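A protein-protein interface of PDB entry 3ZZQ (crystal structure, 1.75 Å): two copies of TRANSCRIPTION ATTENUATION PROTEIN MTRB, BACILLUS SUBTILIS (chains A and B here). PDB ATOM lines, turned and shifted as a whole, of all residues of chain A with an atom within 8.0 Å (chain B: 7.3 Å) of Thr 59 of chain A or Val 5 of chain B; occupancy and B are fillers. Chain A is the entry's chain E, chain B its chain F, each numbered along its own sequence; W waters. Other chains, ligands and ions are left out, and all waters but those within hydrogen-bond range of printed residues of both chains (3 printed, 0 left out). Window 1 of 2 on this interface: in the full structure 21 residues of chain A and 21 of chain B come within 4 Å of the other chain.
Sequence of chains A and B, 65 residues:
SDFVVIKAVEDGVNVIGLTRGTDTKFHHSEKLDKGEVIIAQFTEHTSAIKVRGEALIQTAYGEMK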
ATOM      1  N   ASP A   2      28.484  23.098 -15.666  1.00  0.00           N
ATOM      2  CA  ASP A   2      27.943  22.947 -14.327  1.00  0.00           C
ATOM      3  C   ASP A   2      27.853  24.331 -13.679  1.00  0.00           C
ATOM      4  O   ASP A   2      28.578  25.257 -14.056  1.00  0.00           O
ATOM      5  CB  ASP A   2      28.801  21.984 -13.504  1.00  0.00           C
ATOM      6  CG  ASP A   2      28.684  20.542 -13.989  1.00  0.00           C
ATOM      7  OD1 ASP A   2      27.614  20.179 -14.524  1.00  0.00           O
ATOM      8  OD2 ASP A   2      29.648  19.771 -13.831  1.00  0.00           O
ATOM      9  N   PHE A   3      26.918  24.481 -12.755  1.00  0.00           N
ATOM     10  CA  PHE A   3      26.740  25.744 -12.048  1.00  0.00           C
ATOM     11  C   PHE A   3      26.371  25.493 -10.594  1.00  0.00           C
ATOM     12  O   PHE A   3      26.144  24.346 -10.179  1.00  0.00           O
ATOM     13  CB  PHE A   3      25.693  26.621 -12.744  1.00  0.00           C
ATOM     14  CG  PHE A   3      24.309  26.040 -12.747  1.00  0.00           C
ATOM     15  CD1 PHE A   3      23.931  25.129 -13.719  1.00  0.00           C
ATOM     16  CD2 PHE A   3      23.383  26.410 -11.782  1.00  0.00           C
ATOM     17  CE1 PHE A   3      22.642  24.593 -13.730  1.00  0.00           C
ATOM     18  CE2 PHE A   3      22.105  25.878 -11.784  1.00  0.00           C
ATOM     19  CZ  PHE A   3      21.734  24.968 -12.754  1.00  0.00           C
ATOM     20  N   VAL A   4      26.358  26.573  -9.826  1.00  0.00           N
ATOM     21  CA  VAL A   4      26.055  26.556  -8.398  1.00  0.00           C
ATOM     22  C   VAL A   4      24.990  27.623  -8.148  1.00  0.00           C
ATOM     23  O   VAL A   4      25.023  28.688  -8.779  1.00  0.00           O
ATOM     24  CB  VAL A   4      27.317  26.895  -7.551  1.00  0.00           C
ATOM     25  CG1 VAL A   4      27.058  26.673  -6.057  1.00  0.00           C
ATOM     26  CG2 VAL A   4      28.525  26.077  -8.014  1.00  0.00           C
ATOM     27  N   VAL A   5      24.068  27.350  -7.235  1.00  0.00           N
ATOM     28  CA  VAL A   5      23.079  28.325  -6.810  1.00  0.00           C
ATOM     29  C   VAL A   5      23.390  28.662  -5.364  1.00  0.00           C
ATOM     30  O   VAL A   5      23.492  27.763  -4.522  1.00  0.00           O
ATOM     31  CB  VAL A   5      21.654  27.762  -6.900  1.00  0.00           C
ATOM     32  CG1 VAL A   5      20.647  28.852  -6.618  1.00  0.00           C
ATOM     33  CG2 VAL A   5      21.405  27.133  -8.271  1.00  0.00           C
ATOM     34  N   ILE A   6      23.559  29.947  -5.078  1.00  0.00           N
ATOM     35  CA  ILE A   6      23.930  30.400  -3.736  1.00  0.00           C
ATOM     36  C   ILE A   6      22.938  31.464  -3.286  1.00  0.00           C
ATOM     37  O   ILE A   6      22.763  32.480  -3.967  1.00  0.00           O
ATOM     38  CB  ILE A   6      25.357  30.982  -3.719  1.00  0.00           C
ATOM     39  CG1 ILE A   6      26.373  29.937  -4.175  1.00  0.00           C
ATOM     40  CG2 ILE A   6      25.709  31.510  -2.317  1.00  0.00           C
ATOM     41  CD1 ILE A   6      27.529  30.500  -4.974  1.00  0.00           C
ATOM     42  N   PHE A  42      30.730  27.376 -13.669  1.00  0.00           N
ATOM     43  CA  PHE A  42      32.136  27.154 -13.933  1.00  0.00           C
ATOM     44  C   PHE A  42      32.380  27.513 -15.380  1.00  0.00           C
ATOM     45  O   PHE A  42      31.527  27.272 -16.240  1.00  0.00           O
ATOM     46  CB  PHE A  42      32.514  25.706 -13.631  1.00  0.00           C
ATOM     47  CG  PHE A  42      32.477  25.395 -12.172  1.00  0.00           C
ATOM     48  CD1 PHE A  42      33.430  25.931 -11.325  1.00  0.00           C
ATOM     49  CD2 PHE A  42      31.480  24.598 -11.634  1.00  0.00           C
ATOM     50  CE1 PHE A  42      33.392  25.671  -9.964  1.00  0.00           C
ATOM     51  CE2 PHE A  42      31.441  24.336 -10.267  1.00  0.00           C
ATOM     52  CZ  PHE A  42      32.406  24.872  -9.440  1.00  0.00           C
ATOM     53  N   ILE A  49      34.938  27.859  -6.741  1.00  0.00           N
ATOM     54  CA  ILE A  49      34.117  28.932  -6.182  1.00  0.00           C
ATOM     55  C   ILE A  49      34.131  28.773  -4.673  1.00  0.00           C
ATOM     56  O   ILE A  49      33.890  27.678  -4.170  1.00  0.00           O
ATOM     57  CB  ILE A  49      32.659  28.861  -6.690  1.00  0.00           C
ATOM     58  CG1 ILE A  49      32.600  29.116  -8.197  1.00  0.00           C
ATOM     59  CG2 ILE A  49      31.783  29.895  -5.958  1.00  0.00           C
ATOM     60  CD1 ILE A  49      31.243  28.787  -8.851  1.00  0.00           C
ATOM     61  N   LEU A  56      22.719  29.285   1.655  1.00  0.00           N
ATOM     62  CA  LEU A  56      22.091  28.061   1.195  1.00  0.00           C
ATOM     63  C   LEU A  56      22.672  27.785  -0.181  1.00  0.00           C
ATOM     64  O   LEU A  56      22.683  28.672  -1.032  1.00  0.00           O
ATOM     65  CB  LEU A  56      20.580  28.252   1.110  1.00  0.00           C
ATOM     66  CG  LEU A  56      19.720  27.165   0.466  1.00  0.00           C
ATOM     67  CD1 LEU A  56      19.972  25.822   1.124  1.00  0.00           C
ATOM     68  CD2 LEU A  56      18.245  27.565   0.569  1.00  0.00           C
ATOM     69  N   ILE A  57      23.163  26.570  -0.397  1.00  0.00           N
ATOM     70  CA  ILE A  57      23.823  26.234  -1.657  1.00  0.00           C
ATOM     71  C   ILE A  57      23.191  25.009  -2.294  1.00  0.00           C
ATOM     72  O   ILE A  57      22.960  23.999  -1.623  1.00  0.00           O
ATOM     73  CB  ILE A  57      25.324  26.000  -1.445  1.00  0.00           C
ATOM     74  CG1 ILE A  57      25.991  27.291  -0.953  1.00  0.00           C
ATOM     75  CG2 ILE A  57      25.996  25.501  -2.736  1.00  0.00           C
ATOM     76  CD1 ILE A  57      27.367  27.084  -0.386  1.00  0.00           C
ATOM     77  N   GLN A  58      22.909  25.107  -3.589  1.00  0.00           N
ATOM     78  CA  GLN A  58      22.429  23.973  -4.370  1.00  0.00           C
ATOM     79  C   GLN A  58      23.369  23.691  -5.533  1.00  0.00           C
ATOM     80  O   GLN A  58      23.782  24.613  -6.233  1.00  0.00           O
ATOM     81  CB  GLN A  58      21.042  24.251  -4.940  1.00  0.00           C
ATOM     82  CG  GLN A  58      19.957  24.457  -3.920  1.00  0.00           C
ATOM     83  CD  GLN A  58      18.623  24.826  -4.565  1.00  0.00           C
ATOM     84  OE1 GLN A  58      18.583  25.371  -5.672  1.00  0.00           O
ATOM     85  NE2 GLN A  58      17.528  24.533  -3.869  1.00  0.00           N
ATOM     86  N   THR A  59      23.690  22.416  -5.744  1.00  0.00           N
ATOM     87  CA  THR A  59      24.429  21.984  -6.921  1.00  0.00           C
ATOM     88  C   THR A  59      23.749  20.755  -7.502  1.00  0.00           C
ATOM     89  O   THR A  59      22.742  20.292  -6.968  1.00  0.00           O
ATOM     90  CB  THR A  59      25.879  21.609  -6.579  1.00  0.00           C
ATOM     91  OG1 THR A  59      25.891  20.398  -5.812  1.00  0.00           O
ATOM     92  CG2 THR A  59      26.567  22.743  -5.805  1.00  0.00           C
ATOM     93  N   ALA A  60      24.321  20.217  -8.576  1.00  0.00           N
ATOM     94  CA  ALA A  60      23.857  18.949  -9.147  1.00  0.00           C
ATOM     95  C   ALA A  60      23.798  17.821  -8.114  1.00  0.00           C
ATOM     96  O   ALA A  60      23.025  16.871  -8.276  1.00  0.00           O
ATOM     97  CB  ALA A  60      24.752  18.538 -10.317  1.00  0.00           C
ATOM     98  N   TYR A  61      24.609  17.917  -7.060  1.00  0.00           N
ATOM     99  CA  TYR A  61      24.681  16.866  -6.042  1.00  0.00           C
ATOM    100  C   TYR A  61      23.750  17.079  -4.850  1.00  0.00           C
ATOM    101  O   TYR A  61      23.744  16.266  -3.922  1.00  0.00           O
ATOM    102  CB  TYR A  61      26.117  16.710  -5.540  1.00  0.00           C
ATOM    103  CG  TYR A  61      27.149  16.611  -6.634  1.00  0.00           C
ATOM    104  CD1 TYR A  61      26.868  15.985  -7.849  1.00  0.00           C
ATOM    105  CD2 TYR A  61      28.421  17.133  -6.447  1.00  0.00           C
ATOM    106  CE1 TYR A  61      27.828  15.903  -8.852  1.00  0.00           C
ATOM    107  CE2 TYR A  61      29.376  17.051  -7.431  1.00  0.00           C
ATOM    108  CZ  TYR A  61      29.084  16.437  -8.630  1.00  0.00           C
ATOM    109  OH  TYR A  61      30.058  16.361  -9.602  1.00  0.00           O
ATOM    110  N   GLY A  62      22.966  18.153  -4.876  1.00  0.00           N
ATOM    111  CA  GLY A  62      21.980  18.419  -3.827  1.00  0.00           C
ATOM    112  C   GLY A  62      22.236  19.713  -3.080  1.00  0.00           C
ATOM    113  O   GLY A  62      22.847  20.636  -3.614  1.00  0.00           O
ATOM    114  N   GLU A  63      21.787  19.763  -1.828  1.00  0.00           N
ATOM    115  CA  GLU A  63      21.747  21.003  -1.062  1.00  0.00           C
ATOM    116  C   GLU A  63      22.728  21.006   0.117  1.00  0.00           C
ATOM    117  O   GLU A  63      22.949  19.977   0.757  1.00  0.00           O
ATOM    118  CB  GLU A  63      20.319  21.237  -0.558  1.00  0.00           C
ATOM    119  CG  GLU A  63      20.005  22.679  -0.190  1.00  0.00           C
ATOM    120  CD  GLU A  63      18.518  22.907   0.065  1.00  0.00           C
ATOM    121  OE1 GLU A  63      17.900  22.078   0.765  1.00  0.00           O
ATOM    122  OE2 GLU A  63      17.969  23.914  -0.432  1.00  0.00           O
ATOM    123  N   MET A  64      23.315  22.173   0.381  1.00  0.00           N
ATOM    124  CA  MET A  64      24.141  22.411   1.570  1.00  0.00           C
ATOM    125  C   MET A  64      23.485  23.510   2.411  1.00  0.00           C
ATOM    126  O   MET A  64      23.267  24.628   1.925  1.00  0.00           O
ATOM    127  CB  MET A  64      25.555  22.852   1.169  1.00  0.00           C
ATOM    128  CG  MET A  64      26.472  21.741   0.672  1.00  0.00           C
ATOM    129  SD  MET A  64      27.500  21.006   1.967  1.00  0.00           S
ATOM    130  CE  MET A  64      28.487  19.865   0.999  1.00  0.00           C
ATOM    131  N   PHE B   3      33.135  17.791 -10.116  1.00  0.00           N
ATOM    132  CA  PHE B   3      33.500  18.724  -9.065  1.00  0.00           C
ATOM    133  C   PHE B   3      33.145  18.142  -7.704  1.00  0.00           C
ATOM    134  O   PHE B   3      32.450  17.124  -7.619  1.00  0.00           O
ATOM    135  CB  PHE B   3      32.816  20.080  -9.268  1.00  0.00           C
ATOM    136  CG  PHE B   3      31.323  20.027  -9.175  1.00  0.00           C
ATOM    137  CD1 PHE B   3      30.557  19.769 -10.305  1.00  0.00           C
ATOM    138  CD2 PHE B   3      30.681  20.225  -7.960  1.00  0.00           C
ATOM    139  CE1 PHE B   3      29.174  19.710 -10.224  1.00  0.00           C
ATOM    140  CE2 PHE B   3      29.297  20.169  -7.867  1.00  0.00           C
ATOM    141  CZ  PHE B   3      28.543  19.905  -8.994  1.00  0.00           C
ATOM    142  N   VAL B   4      33.661  18.778  -6.661  1.00  0.00           N
ATOM    143  CA  VAL B   4      33.353  18.368  -5.304  1.00  0.00           C
ATOM    144  C   VAL B   4      32.894  19.574  -4.510  1.00  0.00           C
ATOM    145  O   VAL B   4      33.303  20.703  -4.775  1.00  0.00           O
ATOM    146  CB  VAL B   4      34.548  17.702  -4.618  1.00  0.00           C
ATOM    147  CG1 VAL B   4      34.933  16.422  -5.358  1.00  0.00           C
ATOM    148  CG2 VAL B   4      35.725  18.668  -4.517  1.00  0.00           C
ATOM    149  N   VAL B   5      31.993  19.330  -3.559  1.00  0.00           N
ATOM    150  CA  VAL B   5      31.504  20.386  -2.677  1.00  0.00           C
ATOM    151  C   VAL B   5      32.045  20.071  -1.292  1.00  0.00           C
ATOM    152  O   VAL B   5      31.863  18.954  -0.801  1.00  0.00           O
ATOM    153  CB  VAL B   5      29.971  20.433  -2.625  1.00  0.00           C
ATOM    154  CG1 VAL B   5      29.495  21.629  -1.814  1.00  0.00           C
ATOM    155  CG2 VAL B   5      29.389  20.480  -4.037  1.00  0.00           C
ATOM    156  N   ILE B   6      32.713  21.042  -0.682  1.00  0.00           N
ATOM    157  CA  ILE B   6      33.360  20.867   0.621  1.00  0.00           C
ATOM    158  C   ILE B   6      32.920  21.984   1.565  1.00  0.00           C
ATOM    159  O   ILE B   6      33.146  23.167   1.287  1.00  0.00           O
ATOM    160  CB  ILE B   6      34.906  20.865   0.482  1.00  0.00           C
ATOM    161  CG1 ILE B   6      35.353  19.755  -0.474  1.00  0.00           C
ATOM    162  CG2 ILE B   6      35.573  20.700   1.863  1.00  0.00           C
ATOM    163  CD1 ILE B   6      36.673  20.007  -1.185  1.00  0.00           C
ATOM    164  N   LYS B   7      32.279  21.612   2.674  1.00  0.00           N
ATOM    165  CA  LYS B   7      31.863  22.577   3.694  1.00  0.00           C
ATOM    166  C   LYS B   7      32.587  22.273   5.001  1.00  0.00           C
ATOM    167  O   LYS B   7      32.587  21.132   5.454  1.00  0.00           O
ATOM    168  CB  LYS B   7      30.345  22.528   3.908  1.00  0.00           C
ATOM    169  CG  LYS B   7      29.833  23.507   4.947  1.00  0.00           C
ATOM    170  CD  LYS B   7      28.317  23.669   4.879  1.00  0.00           C
ATOM    171  CE  LYS B   7      27.834  24.686   5.899  1.00  0.00           C
ATOM    172  NZ  LYS B   7      26.403  25.042   5.709  1.00  0.00           N
ATOM    173  N   VAL B  37      32.395  27.261   2.374  1.00  0.00           N
ATOM    174  CA  VAL B  37      32.250  26.220   1.370  1.00  0.00           C
ATOM    175  C   VAL B  37      33.176  26.499   0.193  1.00  0.00           C
ATOM    176  O   VAL B  37      33.366  27.656  -0.191  1.00  0.00           O
ATOM    177  CB  VAL B  37      30.788  26.156   0.853  1.00  0.00           C
ATOM    178  CG1 VAL B  37      30.649  25.143  -0.284  1.00  0.00           C
ATOM    179  CG2 VAL B  37      29.829  25.832   1.992  1.00  0.00           C
ATOM    180  N   ILE B  38      33.761  25.444  -0.360  1.00  0.00           N
ATOM    181  CA  ILE B  38      34.396  25.527  -1.676  1.00  0.00           C
ATOM    182  C   ILE B  38      33.774  24.485  -2.600  1.00  0.00           C
ATOM    183  O   ILE B  38      33.527  23.344  -2.198  1.00  0.00           O
ATOM    184  CB  ILE B  38      35.941  25.420  -1.616  1.00  0.00           C
ATOM    185  CG1 ILE B  38      36.548  25.668  -3.007  1.00  0.00           C
ATOM    186  CG2 ILE B  38      36.393  24.080  -1.058  1.00  0.00           C
ATOM    187  CD1 ILE B  38      37.970  26.246  -2.967  1.00  0.00           C
ATOM    188  N   ILE B  39      33.453  24.918  -3.819  1.00  0.00           N
ATOM    189  CA  ILE B  39      32.988  24.026  -4.874  1.00  0.00           C
ATOM    190  C   ILE B  39      34.105  24.052  -5.903  1.00  0.00           C
ATOM    191  O   ILE B  39      34.396  25.102  -6.473  1.00  0.00           O
ATOM    192  CB  ILE B  39      31.653  24.459  -5.515  1.00  0.00           C
ATOM    193  CG1 ILE B  39      30.594  24.774  -4.447  1.00  0.00           C
ATOM    194  CG2 ILE B  39      31.140  23.342  -6.428  1.00  0.00           C
ATOM    195  CD1 ILE B  39      30.503  26.244  -4.077  1.00  0.00           C
ATOM    196  N   ALA B  40      34.783  22.920  -6.073  1.00  0.00           N
ATOM    197  CA  ALA B  40      36.016  22.882  -6.860  1.00  0.00           C
ATOM    198  C   ALA B  40      35.977  21.780  -7.894  1.00  0.00           C
ATOM    199  O   ALA B  40      35.608  20.638  -7.596  1.00  0.00           O
ATOM    200  CB  ALA B  40      37.218  22.683  -5.938  1.00  0.00           C
ATOM    201  N   ALA B  55      35.044  18.084   7.649  1.00  0.00           N
ATOM    202  CA  ALA B  55      34.292  18.703   6.574  1.00  0.00           C
ATOM    203  C   ALA B  55      33.141  17.810   6.152  1.00  0.00           C
ATOM    204  O   ALA B  55      33.177  16.593   6.353  1.00  0.00           O
ATOM    205  CB  ALA B  55      35.207  18.972   5.383  1.00  0.00           C
ATOM    206  N   LEU B  56      32.115  18.436   5.596  1.00  0.00           N
ATOM    207  CA  LEU B  56      31.036  17.738   4.923  1.00  0.00           C
ATOM    208  C   LEU B  56      31.356  17.789   3.433  1.00  0.00           C
ATOM    209  O   LEU B  56      31.602  18.866   2.886  1.00  0.00           O
ATOM    210  CB  LEU B  56      29.713  18.438   5.206  1.00  0.00           C
ATOM    211  CG  LEU B  56      28.459  17.885   4.527  1.00  0.00           C
ATOM    212  CD1 LEU B  56      28.148  16.491   5.045  1.00  0.00           C
ATOM    213  CD2 LEU B  56      27.289  18.833   4.760  1.00  0.00           C
ATOM    214  N   ILE B  57      31.362  16.631   2.784  1.00  0.00           N
ATOM    215  CA  ILE B  57      31.766  16.544   1.381  1.00  0.00           C
ATOM    216  C   ILE B  57      30.667  15.903   0.546  1.00  0.00           C
ATOM    217  O   ILE B  57      30.127  14.861   0.917  1.00  0.00           O
ATOM    218  CB  ILE B  57      33.068  15.759   1.247  1.00  0.00           C
ATOM    219  CG1 ILE B  57      34.204  16.549   1.916  1.00  0.00           C
ATOM    220  CG2 ILE B  57      33.377  15.461  -0.233  1.00  0.00           C
ATOM    221  CD1 ILE B  57      35.485  15.768   2.077  1.00  0.00           C
ATOM    222  N   GLN B  58      30.317  16.555  -0.560  1.00  0.00           N
ATOM    223  CA  GLN B  58      29.365  16.008  -1.518  1.00  0.00           C
ATOM    224  C   GLN B  58      30.021  15.850  -2.877  1.00  0.00           C
ATOM    225  O   GLN B  58      30.702  16.758  -3.355  1.00  0.00           O
ATOM    226  CB  GLN B  58      28.158  16.925  -1.670  1.00  0.00           C
ATOM    227  CG  GLN B  58      27.251  16.988  -0.466  1.00  0.00           C
ATOM    228  CD  GLN B  58      26.096  17.955  -0.672  1.00  0.00           C
ATOM    229  OE1 GLN B  58      26.128  18.798  -1.571  1.00  0.00           O
ATOM    230  NE2 GLN B  58      25.071  17.839   0.164  1.00  0.00           N
ATOM    231  N   THR B  59      29.816  14.694  -3.497  1.00  0.00           N
ATOM    232  CA  THR B  59      30.262  14.478  -4.865  1.00  0.00           C
ATOM    233  C   THR B  59      29.136  13.821  -5.657  1.00  0.00           C
ATOM    234  O   THR B  59      28.062  13.553  -5.114  1.00  0.00           O
ATOM    235  CB  THR B  59      31.511  13.569  -4.903  1.00  0.00           C
ATOM    236  OG1 THR B  59      31.129  12.234  -4.567  1.00  0.00           O
ATOM    237  CG2 THR B  59      32.575  14.058  -3.922  1.00  0.00           C
ATOM    238  N   ALA B  60      29.401  13.524  -6.928  1.00  0.00           N
ATOM    239  CA  ALA B  60      28.470  12.759  -7.758  1.00  0.00           C
ATOM    240  C   ALA B  60      28.087  11.408  -7.145  1.00  0.00           C
ATOM    241  O   ALA B  60      27.047  10.852  -7.498  1.00  0.00           O
ATOM    242  CB  ALA B  60      29.054  12.545  -9.154  1.00  0.00           C
ATOM    243  N   GLY B  62      27.701  10.809  -3.789  1.00  0.00           N
ATOM    244  CA  GLY B  62      26.953  10.967  -2.546  1.00  0.00           C
ATOM    245  C   GLY B  62      27.681  11.794  -1.508  1.00  0.00           C
ATOM    246  O   GLY B  62      28.589  12.555  -1.829  1.00  0.00           O
ATOM    247  N   MET B  64      29.865  12.413   2.053  1.00  0.00           N
ATOM    248  CA  MET B  64      30.930  11.870   2.883  1.00  0.00           C
ATOM    249  C   MET B  64      31.029  12.776   4.112  1.00  0.00           C
ATOM    250  O   MET B  64      31.497  13.914   4.022  1.00  0.00           O
ATOM    251  CB  MET B  64      32.242  11.837   2.078  1.00  0.00           C
ATOM    252  CG  MET B  64      33.456  11.237   2.789  1.00  0.00           C
ATOM    253  SD  MET B  64      33.389   9.445   3.023  1.00  0.00           S
ATOM    254  CE  MET B  64      33.802   8.828   1.394  1.00  0.00           C
HETATM  255  O   HOH W   1      31.696  14.699  -8.411  1.00  0.00           O
HETATM  256  O   HOH W   2      25.644  20.844  -3.185  1.00  0.00           O
HETATM  257  O   HOH W   3      25.845  25.671   2.960  1.00  0.00           O
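The backbone carbonyl oxygen (O) of Phe 3 of chain B lies close to the side-chain hydroxyl (OH) of Tyr 61 of chain A (3.2 Å). The backbone NH (N) of Ile 39 of chain B sits at hydrogen-bond distance from the backbone carbonyl oxygen (O) of Ile 49 of chain A (2.8 Å). NE2 of Gln 58 of chain B lies within hydrogen-bond range of O of Glu 63 of chain A (3.1 Å).
N of Leu 56 of chain B is in hydrogen-bond range of O of Lys 7 of chain B (2.7 Å). O of Asp 2 of chain A lies within hydrogen-bond range of N of Phe 42 of chain A, 3.0 Å away. N of Gln 58 of chain B sits at hydrogen-bond distance from O of Val 5 of chain B. The backbone NH (N) of Ile 6 of chain B is in hydrogen-bond range of the backbone carbonyl oxygen (O) of Ile 38 of chain B, at 2.9 Å. The side-chain hydroxyl of Thr 59 of chain A sits close to the backbone NH of Tyr 61 of chain A (3.1 Å). O of Ile 57 of chain A sits at hydrogen-bond distance from N of Met 64 of chain A (2.7 Å).
Among the printed residues, merely in contact across the chains: Asp 2 of chain A with Phe 3 of chain B (3.6 Å), Val 4 of chain A with Ile 39 of chain B (3.997 Å), Phe 42 of chain A with Ile 39 of chain B (3.6 Å), Ile 49 of chain A with Ile 38 of chain B (3.3 Å), Ile 57 of chain A with Val 37 of chain B (3.6 Å), Thr 59 of chain A with Phe 3 of chain B (3.9 Å), Thr 59 of chain A with Val 5 of chain B (3.9 Å), Tyr 61 of chain A with Gln 58 of chain B (3.9 Å), Tyr 61 of chain A with Thr 59 of chain B (3.5 Å), Tyr 61 of chain A with Ala 60 of chain B (3.4 Å), Met 64 of chain A with Val 5 of chain B (3.5 Å), Met 64 of chain A with Lys 7 of chain B (3.8 Å), Met 64 of chain A with Leu 56 of chain B (3.5 Å) and Met 64 of chain A with Gln 58 of chain B (3.5 Å).
Thr 59 of chain A touches just these residues of chain B: Phe 3 and Val 5. Val 5 of chain B touches just these residues of chain A: Thr 59 (3.9 Å) and Met 64 (3.5 Å). Of the printed residues of chain A, Ile 38 of chain B touches Ile 49 (3.3 Å). Of the printed residues of chain B, Ile 49 of chain A touches Ile 38 and Ile 39. Phe 3 of chain A touches none of the printed residues of chain B. The nearest residue of chain B that does not touch Thr 59 of chain A is Gln 58 of chain B (4.5 Å). The nearest residue of chain A that does not touch Val 5 of chain B is Tyr 61 of chain A (4.2 Å). The nearest printed residue of chain A that does not touch Thr 59 of chain B is Ala 60 of chain A (6.7 Å).
Of the 16 printed residues of chain A, 9 touch a printed residue of chain B. Hydrophobic or aromatic side chains of chain A within 4 Å of the printed part of chain B: Val 4, Phe 42, Ile 57, Tyr 61 and Met 64. Of the 17 printed residues of chain B, 10 touch a printed residue of chain A.
Thr 59 of chain A touches Phe 3 of chain B, but with the chains exchanged Phe 3 of chain A does not touch Thr 59 of chain B (11.8 Å). Thr 59 of chain A touches Val 5 of chain B, but with the chains exchanged Val 5 of chain A does not touch Thr 59 of chain B (14.4 Å). Met 64 of chain A touches Val 5 of chain B, but with the chains exchanged Val 5 of chain A does not touch Met 64 of chain B (17.9 Å). Met 64 of chain A touches Leu 56 of chain B, but with the chains exchanged Leu 56 of chain A does not touch Met 64 of chain B (16.7 Å). 11 positions are printed for both chains. Of the 17 pairs that touch across the chains among the printed residues, none has its exchanged pair printed and touching as well.
Water W1 lies within hydrogen-bond range of the side-chain hydroxyl of Tyr 61 of chain A (2.6 Å), the backbone carbonyl oxygen of Phe 3 of chain B (2.7 Å) and the backbone NH of Ala 60 of chain B (3.0 Å). Water W2 lies within hydrogen-bond range of OE1 of Gln 58 of chain B (2.7 Å), OG1 of Thr 59 of chain A (2.7 Å) and O of Gly 62 of chain A (2.8 Å). Water W3 lies within hydrogen-bond range of the side-chain amino group of Lys 7 of chain B (2.9 Å) and the backbone carbonyl oxygen of Met 64 of chain A (3.0 Å).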
